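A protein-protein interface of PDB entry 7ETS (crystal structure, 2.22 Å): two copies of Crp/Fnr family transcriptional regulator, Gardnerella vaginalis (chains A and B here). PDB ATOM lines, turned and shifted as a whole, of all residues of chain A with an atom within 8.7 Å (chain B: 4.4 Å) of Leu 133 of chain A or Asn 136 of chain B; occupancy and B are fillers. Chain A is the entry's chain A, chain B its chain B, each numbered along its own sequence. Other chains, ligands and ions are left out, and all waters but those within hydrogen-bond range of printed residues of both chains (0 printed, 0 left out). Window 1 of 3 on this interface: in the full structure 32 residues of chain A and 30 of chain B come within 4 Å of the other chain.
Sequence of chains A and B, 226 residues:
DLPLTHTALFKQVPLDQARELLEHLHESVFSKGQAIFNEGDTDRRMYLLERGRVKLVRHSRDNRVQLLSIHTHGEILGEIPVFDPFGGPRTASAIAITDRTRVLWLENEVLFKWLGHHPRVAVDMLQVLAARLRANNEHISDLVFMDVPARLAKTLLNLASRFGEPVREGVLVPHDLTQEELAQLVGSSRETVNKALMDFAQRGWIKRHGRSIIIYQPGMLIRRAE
OD1 of Asn 137 of chain B is in hydrogen-bond range of ND2 of Asn 136 of chain A, at 3.5 Å. ND2 of Asn 137 of chain B lies within hydrogen-bond range of OE2 of Glu 79 of chain A, at 2.6 Å.
O of Leu 133 of chain A lies within hydrogen-bond range of ND2 of Asn 137 of chain A.
Leu 133 of chain B touches Glu 79 of chain A (CD2 to OE1, 3.9 Å). CB of Glu 79 of chain A touches NE of Arg 134 of chain B, at 3.2 Å. CG of Glu 138 of chain B touches CG2 of Thr 91 of chain A (3.8 Å). Arg 132 of chain B touches Leu 133 of chain A (CG to CD2, 3.8 Å). Leu 133 of chain A touches Asn 136 of chain B (CD1 to OD1, 3.3 Å). Asn 136 of chain B touches Asn 136 of chain A (CB to OD1, 3.1 Å). CD2 of His 139 of chain A touches CD1 of Ile 140 of chain B (3.7 Å). ND2 of Asn 136 of chain B touches CD1 of Ile 140 of chain A (3.5 Å). CG2 of Ile 140 of chain A touches NE2 of His 139 of chain B, at 3.5 Å. CG1 of Ile 140 of chain B touches CG1 of Ile 140 of chain A, 3.7 Å away.
Printed residues of chain B within 4 Å of Leu 133 of chain A: Arg 132 and Asn 136. Of the printed residues of chain A, Asn 137 of chain B touches Glu 79 and Asn 136. Of the printed residues of chain A, Ile 140 of chain B touches His 139 (3.7 Å) and Ile 140 (3.7 Å). The nearest residue of chain A that does not touch Asn 136 of chain B is Asn 137 of chain A (4.1 Å).
Of the 10 printed residues of chain B, 8 touch a printed residue of chain A. Of the 21 printed residues of chain A, 6 touch a printed residue of chain B. Hydrophobic or aromatic side chains of chain A within 4 Å of the printed part of chain B: Leu 133, His 139 and Ile 140. Along chain A the printed residues that touch a printed residue of chain B span positions 79 to 140. Among the printed residues, 12 pairs touch across the chains. Among the printed residues, no Asp or Glu carboxylate lies within 4 Å of a Lys or Arg side-chain nitrogen of the other chain.
Leu 133 of chain A touches Asn 136 of chain B, but with the chains exchanged Asn 136 of chain A does not touch Leu 133 of chain B (4.3 Å). Asn 136 of chain A touches its own counterpart, Asn 136 of chain B. His 139 of chain A touches Ile 140 of chain B, and with the chains exchanged Ile 140 of chain A touches His 139 of chain B. Ile 140 of chain A touches Asn 136 of chain B, but with the chains exchanged Asn 136 of chain A does not touch Ile 140 of chain B (4.03 Å). 10 positions are printed for both chains. Of the 12 pairs that touch across the chains among the printed residues, 4 have their exchanged pair printed and touching as well.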
ATOM      1  N   ASP A   1     -10.008  -2.244  20.372  1.00  0.00           N
ATOM      2  CA  ASP A   1     -10.215  -0.808  20.502  1.00  0.00           C
ATOM      3  C   ASP A   1     -11.196  -0.479  21.624  1.00  0.00           C
ATOM      4  O   ASP A   1     -11.246  -1.169  22.643  1.00  0.00           O
ATOM      5  CB  ASP A   1     -10.720  -0.215  19.183  1.00  0.00           C
ATOM      6  CG  ASP A   1      -9.660  -0.211  18.097  1.00  0.00           C
ATOM      7  OD1 ASP A   1      -8.466  -0.031  18.422  1.00  0.00           O
ATOM      8  OD2 ASP A   1     -10.024  -0.382  16.916  1.00  0.00           O
ATOM      9  N   LEU A   2     -11.978   0.583  21.421  1.00  0.00           N
ATOM     10  CA  LEU A   2     -12.931   1.213  22.330  1.00  0.00           C
ATOM     11  C   LEU A   2     -14.335   0.646  22.115  1.00  0.00           C
ATOM     12  O   LEU A   2     -14.735   0.395  20.975  1.00  0.00           O
ATOM     13  CB  LEU A   2     -12.951   2.728  22.126  1.00  0.00           C
ATOM     14  CG  LEU A   2     -11.710   3.542  22.521  1.00  0.00           C
ATOM     15  CD1 LEU A   2     -10.575   3.390  21.513  1.00  0.00           C
ATOM     16  CD2 LEU A   2     -12.058   5.013  22.708  1.00  0.00           C
ATOM     17  N   LEU A   4     -18.606   0.142  22.152  1.00  0.00           N
ATOM     18  CA  LEU A   4     -19.676   0.839  21.447  1.00  0.00           C
ATOM     19  C   LEU A   4     -20.121   2.075  22.214  1.00  0.00           C
ATOM     20  O   LEU A   4     -20.319   2.027  23.431  1.00  0.00           O
ATOM     21  CB  LEU A   4     -20.868  -0.096  21.242  1.00  0.00           C
ATOM     22  CG  LEU A   4     -21.059  -0.730  19.865  1.00  0.00           C
ATOM     23  CD1 LEU A   4     -21.258   0.347  18.815  1.00  0.00           C
ATOM     24  CD2 LEU A   4     -19.881  -1.620  19.514  1.00  0.00           C
ATOM     25  N   GLU A  79     -24.760  -5.915  24.912  1.00  0.00           N
ATOM     26  CA  GLU A  79     -24.856  -6.181  23.489  1.00  0.00           C
ATOM     27  C   GLU A  79     -26.095  -5.530  22.886  1.00  0.00           C
ATOM     28  O   GLU A  79     -27.050  -5.182  23.584  1.00  0.00           O
ATOM     29  CB  GLU A  79     -24.884  -7.686  23.237  1.00  0.00           C
ATOM     30  CG  GLU A  79     -23.932  -8.468  24.122  1.00  0.00           C
ATOM     31  CD  GLU A  79     -22.481  -8.099  23.885  1.00  0.00           C
ATOM     32  OE1 GLU A  79     -22.138  -7.741  22.738  1.00  0.00           O
ATOM     33  OE2 GLU A  79     -21.685  -8.162  24.846  1.00  0.00           O
ATOM     34  N   THR A  91     -24.910 -12.130  28.380  1.00  0.00           N
ATOM     35  CA  THR A  91     -23.653 -12.820  28.640  1.00  0.00           C
ATOM     36  C   THR A  91     -23.010 -12.402  29.956  1.00  0.00           C
ATOM     37  O   THR A  91     -22.117 -13.105  30.442  1.00  0.00           O
ATOM     38  CB  THR A  91     -22.667 -12.575  27.495  1.00  0.00           C
ATOM     39  OG1 THR A  91     -22.233 -11.210  27.520  1.00  0.00           O
ATOM     40  CG2 THR A  91     -23.323 -12.864  26.154  1.00  0.00           C
ATOM     41  N   LEU A 126     -24.073  -0.789  10.290  1.00  0.00           N
ATOM     42  CA  LEU A 126     -23.400  -2.010   9.868  1.00  0.00           C
ATOM     43  C   LEU A 126     -21.895  -1.797   9.765  1.00  0.00           C
ATOM     44  O   LEU A 126     -21.112  -2.692  10.106  1.00  0.00           O
ATOM     45  CB  LEU A 126     -23.976  -2.485   8.534  1.00  0.00           C
ATOM     46  CG  LEU A 126     -23.723  -3.944   8.150  1.00  0.00           C
ATOM     47  CD1 LEU A 126     -24.250  -4.869   9.231  1.00  0.00           C
ATOM     48  CD2 LEU A 126     -24.375  -4.253   6.814  1.00  0.00           C
ATOM     49  N   GLN A 127     -21.470  -0.618   9.301  1.00  0.00           N
ATOM     50  CA  GLN A 127     -20.046  -0.303   9.265  1.00  0.00           C
ATOM     51  C   GLN A 127     -19.453  -0.171  10.661  1.00  0.00           C
ATOM     52  O   GLN A 127     -18.239  -0.337  10.823  1.00  0.00           O
ATOM     53  CB  GLN A 127     -19.795   0.987   8.480  1.00  0.00           C
ATOM     54  CG  GLN A 127     -20.139   0.905   7.003  1.00  0.00           C
ATOM     55  CD  GLN A 127     -19.436   1.971   6.181  1.00  0.00           C
ATOM     56  OE1 GLN A 127     -18.376   2.469   6.564  1.00  0.00           O
ATOM     57  NE2 GLN A 127     -20.024   2.326   5.044  1.00  0.00           N
ATOM     58  N   VAL A 128     -20.276   0.124  11.667  1.00  0.00           N
ATOM     59  CA  VAL A 128     -19.777   0.220  13.034  1.00  0.00           C
ATOM     60  C   VAL A 128     -19.596  -1.166  13.638  1.00  0.00           C
ATOM     61  O   VAL A 128     -18.565  -1.458  14.254  1.00  0.00           O
ATOM     62  CB  VAL A 128     -20.715   1.096  13.883  1.00  0.00           C
ATOM     63  CG1 VAL A 128     -20.400   0.933  15.358  1.00  0.00           C
ATOM     64  CG2 VAL A 128     -20.585   2.556  13.471  1.00  0.00           C
ATOM     65  N   LEU A 129     -20.592  -2.041  13.471  1.00  0.00           N
ATOM     66  CA  LEU A 129     -20.444  -3.419  13.927  1.00  0.00           C
ATOM     67  C   LEU A 129     -19.337  -4.132  13.167  1.00  0.00           C
ATOM     68  O   LEU A 129     -18.666  -5.011  13.722  1.00  0.00           O
ATOM     69  CB  LEU A 129     -21.762  -4.178  13.772  1.00  0.00           C
ATOM     70  CG  LEU A 129     -22.996  -3.654  14.512  1.00  0.00           C
ATOM     71  CD1 LEU A 129     -24.014  -4.772  14.674  1.00  0.00           C
ATOM     72  CD2 LEU A 129     -22.625  -3.061  15.861  1.00  0.00           C
ATOM     73  N   ALA A 130     -19.134  -3.767  11.898  1.00  0.00           N
ATOM     74  CA  ALA A 130     -18.036  -4.333  11.124  1.00  0.00           C
ATOM     75  C   ALA A 130     -16.691  -3.912  11.703  1.00  0.00           C
ATOM     76  O   ALA A 130     -15.823  -4.751  11.973  1.00  0.00           O
ATOM     77  CB  ALA A 130     -18.151  -3.900   9.662  1.00  0.00           C
ATOM     78  N   ALA A 131     -16.506  -2.605  11.905  1.00  0.00           N
ATOM     79  CA  ALA A 131     -15.242  -2.106  12.433  1.00  0.00           C
ATOM     80  C   ALA A 131     -15.005  -2.568  13.865  1.00  0.00           C
ATOM     81  O   ALA A 131     -13.854  -2.670  14.299  1.00  0.00           O
ATOM     82  CB  ALA A 131     -15.209  -0.580  12.352  1.00  0.00           C
ATOM     83  N   ARG A 132     -16.070  -2.853  14.613  1.00  0.00           N
ATOM     84  CA  ARG A 132     -15.908  -3.327  15.981  1.00  0.00           C
ATOM     85  C   ARG A 132     -15.714  -4.834  16.056  1.00  0.00           C
ATOM     86  O   ARG A 132     -15.086  -5.319  17.002  1.00  0.00           O
ATOM     87  CB  ARG A 132     -17.109  -2.921  16.841  1.00  0.00           C
ATOM     88  CG  ARG A 132     -16.825  -2.983  18.332  1.00  0.00           C
ATOM     89  CD  ARG A 132     -15.635  -2.102  18.684  1.00  0.00           C
ATOM     90  NE  ARG A 132     -15.285  -2.169  20.100  1.00  0.00           N
ATOM     91  CZ  ARG A 132     -14.294  -2.905  20.594  1.00  0.00           C
ATOM     92  NH1 ARG A 132     -13.547  -3.647  19.787  1.00  0.00           N
ATOM     93  NH2 ARG A 132     -14.050  -2.900  21.898  1.00  0.00           N
ATOM     94  N   LEU A 133     -16.236  -5.589  15.087  1.00  0.00           N
ATOM     95  CA  LEU A 133     -16.021  -7.030  15.103  1.00  0.00           C
ATOM     96  C   LEU A 133     -14.609  -7.393  14.659  1.00  0.00           C
ATOM     97  O   LEU A 133     -14.033  -8.360  15.171  1.00  0.00           O
ATOM     98  CB  LEU A 133     -17.052  -7.733  14.221  1.00  0.00           C
ATOM     99  CG  LEU A 133     -17.068  -9.263  14.314  1.00  0.00           C
ATOM    100  CD1 LEU A 133     -17.047  -9.711  15.766  1.00  0.00           C
ATOM    101  CD2 LEU A 133     -18.280  -9.837  13.600  1.00  0.00           C
ATOM    102  N   ARG A 134     -14.036  -6.636  13.719  1.00  0.00           N
ATOM    103  CA  ARG A 134     -12.643  -6.865  13.349  1.00  0.00           C
ATOM    104  C   ARG A 134     -11.711  -6.505  14.498  1.00  0.00           C
ATOM    105  O   ARG A 134     -10.713  -7.196  14.738  1.00  0.00           O
ATOM    106  CB  ARG A 134     -12.285  -6.077  12.085  1.00  0.00           C
ATOM    107  CG  ARG A 134     -12.504  -4.577  12.160  1.00  0.00           C
ATOM    108  CD  ARG A 134     -12.047  -3.904  10.871  1.00  0.00           C
ATOM    109  NE  ARG A 134     -10.591  -3.883  10.747  1.00  0.00           N
ATOM    110  CZ  ARG A 134      -9.940  -3.724   9.600  1.00  0.00           C
ATOM    111  NH1 ARG A 134      -8.615  -3.716   9.584  1.00  0.00           N
ATOM    112  NH2 ARG A 134     -10.611  -3.581   8.465  1.00  0.00           N
ATOM    113  N   ALA A 135     -12.029  -5.435  15.230  1.00  0.00           N
ATOM    114  CA  ALA A 135     -11.246  -5.088  16.409  1.00  0.00           C
ATOM    115  C   ALA A 135     -11.438  -6.117  17.515  1.00  0.00           C
ATOM    116  O   ALA A 135     -10.506  -6.408  18.272  1.00  0.00           O
ATOM    117  CB  ALA A 135     -11.626  -3.691  16.898  1.00  0.00           C
ATOM    118  N   ASN A 136     -12.644  -6.679  17.622  1.00  0.00           N
ATOM    119  CA  ASN A 136     -12.887  -7.719  18.615  1.00  0.00           C
ATOM    120  C   ASN A 136     -12.149  -9.004  18.262  1.00  0.00           C
ATOM    121  O   ASN A 136     -11.757  -9.759  19.158  1.00  0.00           O
ATOM    122  CB  ASN A 136     -14.390  -7.976  18.740  1.00  0.00           C
ATOM    123  CG  ASN A 136     -14.722  -8.977  19.827  1.00  0.00           C
ATOM    124  OD1 ASN A 136     -14.669 -10.186  19.608  1.00  0.00           O
ATOM    125  ND2 ASN A 136     -15.073  -8.477  21.007  1.00  0.00           N
ATOM    126  N   ASN A 137     -11.943  -9.263  16.970  1.00  0.00           N
ATOM    127  CA  ASN A 137     -11.240 -10.474  16.561  1.00  0.00           C
ATOM    128  C   ASN A 137      -9.751 -10.387  16.869  1.00  0.00           C
ATOM    129  O   ASN A 137      -9.161 -11.352  17.368  1.00  0.00           O
ATOM    130  CB  ASN A 137     -11.465 -10.734  15.071  1.00  0.00           C
ATOM    131  CG  ASN A 137     -12.701 -11.566  14.805  1.00  0.00           C
ATOM    132  OD1 ASN A 137     -12.936 -12.578  15.465  1.00  0.00           O
ATOM    133  ND2 ASN A 137     -13.502 -11.141  13.834  1.00  0.00           N
ATOM    134  N   GLU A 138      -9.122  -9.245  16.577  1.00  0.00           N
ATOM    135  CA  GLU A 138      -7.704  -9.097  16.877  1.00  0.00           C
ATOM    136  C   GLU A 138      -7.445  -9.048  18.376  1.00  0.00           C
ATOM    137  O   GLU A 138      -6.316  -9.306  18.806  1.00  0.00           O
ATOM    138  CB  GLU A 138      -7.137  -7.854  16.186  1.00  0.00           C
ATOM    139  CG  GLU A 138      -7.881  -6.565  16.481  1.00  0.00           C
ATOM    140  CD  GLU A 138      -7.484  -5.440  15.545  1.00  0.00           C
ATOM    141  OE1 GLU A 138      -8.266  -4.477  15.398  1.00  0.00           O
ATOM    142  OE2 GLU A 138      -6.389  -5.523  14.948  1.00  0.00           O
ATOM    143  N   HIS A 139      -8.465  -8.737  19.178  1.00  0.00           N
ATOM    144  CA  HIS A 139      -8.320  -8.846  20.625  1.00  0.00           C
ATOM    145  C   HIS A 139      -8.289 -10.301  21.070  1.00  0.00           C
ATOM    146  O   HIS A 139      -7.655 -10.626  22.079  1.00  0.00           O
ATOM    147  CB  HIS A 139      -9.457  -8.098  21.325  1.00  0.00           C
ATOM    148  CG  HIS A 139      -9.404  -8.173  22.821  1.00  0.00           C
ATOM    149  ND1 HIS A 139      -8.234  -8.022  23.533  1.00  0.00           N
ATOM    150  CD2 HIS A 139     -10.378  -8.378  23.739  1.00  0.00           C
ATOM    151  CE1 HIS A 139      -8.489  -8.132  24.825  1.00  0.00           C
ATOM    152  NE2 HIS A 139      -9.783  -8.349  24.977  1.00  0.00           N
ATOM    153  N   ILE A 140      -8.961 -11.188  20.333  1.00  0.00           N
ATOM    154  CA  ILE A 140      -8.956 -12.607  20.678  1.00  0.00           C
ATOM    155  C   ILE A 140      -7.622 -13.246  20.317  1.00  0.00           C
ATOM    156  O   ILE A 140      -7.080 -14.054  21.080  1.00  0.00           O
ATOM    157  CB  ILE A 140     -10.131 -13.322  19.989  1.00  0.00           C
ATOM    158  CG1 ILE A 140     -11.457 -12.676  20.398  1.00  0.00           C
ATOM    159  CG2 ILE A 140     -10.130 -14.804  20.333  1.00  0.00           C
ATOM    160  CD1 ILE A 140     -12.660 -13.256  19.690  1.00  0.00           C
ATOM    161  N   LEU A 143      -4.643 -12.122  23.095  1.00  0.00           N
ATOM    162  CA  LEU A 143      -4.445 -12.808  24.368  1.00  0.00           C
ATOM    163  C   LEU A 143      -3.742 -14.151  24.215  1.00  0.00           C
ATOM    164  O   LEU A 143      -3.344 -14.739  25.227  1.00  0.00           O
ATOM    165  CB  LEU A 143      -5.791 -12.995  25.068  1.00  0.00           C
ATOM    166  CG  LEU A 143      -6.879 -13.682  24.243  1.00  0.00           C
ATOM    167  CD1 LEU A 143      -6.931 -15.179  24.527  1.00  0.00           C
ATOM    168  CD2 LEU A 143      -8.224 -13.020  24.487  1.00  0.00           C
ATOM    169  N   LEU B   4     -18.947 -16.079  10.409  1.00  0.00           N
ATOM    170  CA  LEU B   4     -19.937 -15.600   9.451  1.00  0.00           C
ATOM    171  C   LEU B   4     -19.984 -16.496   8.220  1.00  0.00           C
ATOM    172  O   LEU B   4     -18.950 -16.932   7.711  1.00  0.00           O
ATOM    173  CB  LEU B   4     -19.616 -14.163   9.024  1.00  0.00           C
ATOM    174  CG  LEU B   4     -19.955 -12.991   9.950  1.00  0.00           C
ATOM    175  CD1 LEU B   4     -21.378 -13.110  10.490  1.00  0.00           C
ATOM    176  CD2 LEU B   4     -18.941 -12.878  11.074  1.00  0.00           C
ATOM    177  N   ARG B 132     -23.410 -12.209  16.275  1.00  0.00           N
ATOM    178  CA  ARG B 132     -22.077 -12.775  16.097  1.00  0.00           C
ATOM    179  C   ARG B 132     -21.071 -12.160  17.062  1.00  0.00           C
ATOM    180  O   ARG B 132     -20.194 -12.863  17.575  1.00  0.00           O
ATOM    181  CB  ARG B 132     -21.617 -12.591  14.651  1.00  0.00           C
ATOM    182  CG  ARG B 132     -20.189 -13.039  14.388  1.00  0.00           C
ATOM    183  CD  ARG B 132     -19.962 -14.478  14.820  1.00  0.00           C
ATOM    184  NE  ARG B 132     -18.556 -14.852  14.718  1.00  0.00           N
ATOM    185  CZ  ARG B 132     -17.989 -15.824  15.423  1.00  0.00           C
ATOM    186  NH1 ARG B 132     -16.701 -16.096  15.265  1.00  0.00           N
ATOM    187  NH2 ARG B 132     -18.709 -16.520  16.292  1.00  0.00           N
ATOM    188  N   LEU B 133     -21.179 -10.855  17.329  1.00  0.00           N
ATOM    189  CA  LEU B 133     -20.313 -10.244  18.330  1.00  0.00           C
ATOM    190  C   LEU B 133     -20.656 -10.738  19.730  1.00  0.00           C
ATOM    191  O   LEU B 133     -19.769 -10.831  20.585  1.00  0.00           O
ATOM    192  CB  LEU B 133     -20.405  -8.719  18.246  1.00  0.00           C
ATOM    193  CG  LEU B 133     -19.177  -7.935  18.713  1.00  0.00           C
ATOM    194  CD1 LEU B 133     -19.078  -6.612  17.976  1.00  0.00           C
ATOM    195  CD2 LEU B 133     -19.210  -7.695  20.220  1.00  0.00           C
ATOM    196  N   ARG B 134     -21.929 -11.064  19.978  1.00  0.00           N
ATOM    197  CA  ARG B 134     -22.294 -11.720  21.229  1.00  0.00           C
ATOM    198  C   ARG B 134     -21.563 -13.046  21.385  1.00  0.00           C
ATOM    199  O   ARG B 134     -21.158 -13.418  22.493  1.00  0.00           O
ATOM    200  CB  ARG B 134     -23.805 -11.939  21.286  1.00  0.00           C
ATOM    201  CG  ARG B 134     -24.613 -10.663  21.353  1.00  0.00           C
ATOM    202  CD  ARG B 134     -26.106 -10.946  21.345  1.00  0.00           C
ATOM    203  NE  ARG B 134     -26.854  -9.845  21.943  1.00  0.00           N
ATOM    204  CZ  ARG B 134     -28.177  -9.794  22.038  1.00  0.00           C
ATOM    205  NH1 ARG B 134     -28.924 -10.783  21.566  1.00  0.00           N
ATOM    206  NH2 ARG B 134     -28.755  -8.746  22.604  1.00  0.00           N
ATOM    207  N   ALA B 135     -21.383 -13.773  20.279  1.00  0.00           N
ATOM    208  CA  ALA B 135     -20.716 -15.067  20.341  1.00  0.00           C
ATOM    209  C   ALA B 135     -19.253 -14.915  20.740  1.00  0.00           C
ATOM    210  O   ALA B 135     -18.735 -15.696  21.545  1.00  0.00           O
ATOM    211  CB  ALA B 135     -20.841 -15.782  18.995  1.00  0.00           C
ATOM    212  N   ASN B 136     -18.574 -13.909  20.186  1.00  0.00           N
ATOM    213  CA  ASN B 136     -17.174 -13.683  20.527  1.00  0.00           C
ATOM    214  C   ASN B 136     -17.012 -13.226  21.973  1.00  0.00           C
ATOM    215  O   ASN B 136     -16.014 -13.569  22.619  1.00  0.00           O
ATOM    216  CB  ASN B 136     -16.555 -12.660  19.572  1.00  0.00           C
ATOM    217  CG  ASN B 136     -16.284 -13.236  18.197  1.00  0.00           C
ATOM    218  OD1 ASN B 136     -16.668 -12.656  17.180  1.00  0.00           O
ATOM    219  ND2 ASN B 136     -15.620 -14.383  18.159  1.00  0.00           N
ATOM    220  N   ASN B 137     -17.968 -12.452  22.497  1.00  0.00           N
ATOM    221  CA  ASN B 137     -17.896 -12.054  23.900  1.00  0.00           C
ATOM    222  C   ASN B 137     -18.031 -13.263  24.816  1.00  0.00           C
ATOM    223  O   ASN B 137     -17.376 -13.335  25.863  1.00  0.00           O
ATOM    224  CB  ASN B 137     -18.967 -11.012  24.213  1.00  0.00           C
ATOM    225  CG  ASN B 137     -18.455  -9.591  24.078  1.00  0.00           C
ATOM    226  OD1 ASN B 137     -17.468  -9.335  23.388  1.00  0.00           O
ATOM    227  ND2 ASN B 137     -19.123  -8.658  24.746  1.00  0.00           N
ATOM    228  N   GLU B 138     -18.875 -14.227  24.437  1.00  0.00           N
ATOM    229  CA  GLU B 138     -18.908 -15.499  25.150  1.00  0.00           C
ATOM    230  C   GLU B 138     -17.579 -16.233  25.041  1.00  0.00           C
ATOM    231  O   GLU B 138     -17.183 -16.941  25.974  1.00  0.00           O
ATOM    232  CB  GLU B 138     -20.031 -16.384  24.608  1.00  0.00           C
ATOM    233  CG  GLU B 138     -21.426 -15.987  25.048  1.00  0.00           C
ATOM    234  CD  GLU B 138     -22.471 -17.010  24.638  1.00  0.00           C
ATOM    235  OE1 GLU B 138     -23.046 -16.870  23.537  1.00  0.00           O
ATOM    236  OE2 GLU B 138     -22.706 -17.962  25.411  1.00  0.00           O
ATOM    237  N   HIS B 139     -16.882 -16.079  23.914  1.00  0.00           N
ATOM    238  CA  HIS B 139     -15.618 -16.780  23.721  1.00  0.00           C
ATOM    239  C   HIS B 139     -14.511 -16.175  24.578  1.00  0.00           C
ATOM    240  O   HIS B 139     -13.720 -16.905  25.186  1.00  0.00           O
ATOM    241  CB  HIS B 139     -15.240 -16.764  22.240  1.00  0.00           C
ATOM    242  CG  HIS B 139     -13.867 -17.291  21.957  1.00  0.00           C
ATOM    243  ND1 HIS B 139     -13.600 -18.634  21.797  1.00  0.00           N
ATOM    244  CD2 HIS B 139     -12.683 -16.651  21.804  1.00  0.00           C
ATOM    245  CE1 HIS B 139     -12.310 -18.799  21.561  1.00  0.00           C
ATOM    246  NE2 HIS B 139     -11.732 -17.612  21.560  1.00  0.00           N
ATOM    247  N   ILE B 140     -14.438 -14.844  24.641  1.00  0.00           N
ATOM    248  CA  ILE B 140     -13.455 -14.196  25.503  1.00  0.00           C
ATOM    249  C   ILE B 140     -13.743 -14.504  26.969  1.00  0.00           C
ATOM    250  O   ILE B 140     -12.820 -14.600  27.788  1.00  0.00           O
ATOM    251  CB  ILE B 140     -13.431 -12.680  25.224  1.00  0.00           C
ATOM    252  CG1 ILE B 140     -13.009 -12.419  23.777  1.00  0.00           C
ATOM    253  CG2 ILE B 140     -12.487 -11.963  26.180  1.00  0.00           C
ATOM    254  CD1 ILE B 140     -12.987 -10.954  23.403  1.00  0.00           C
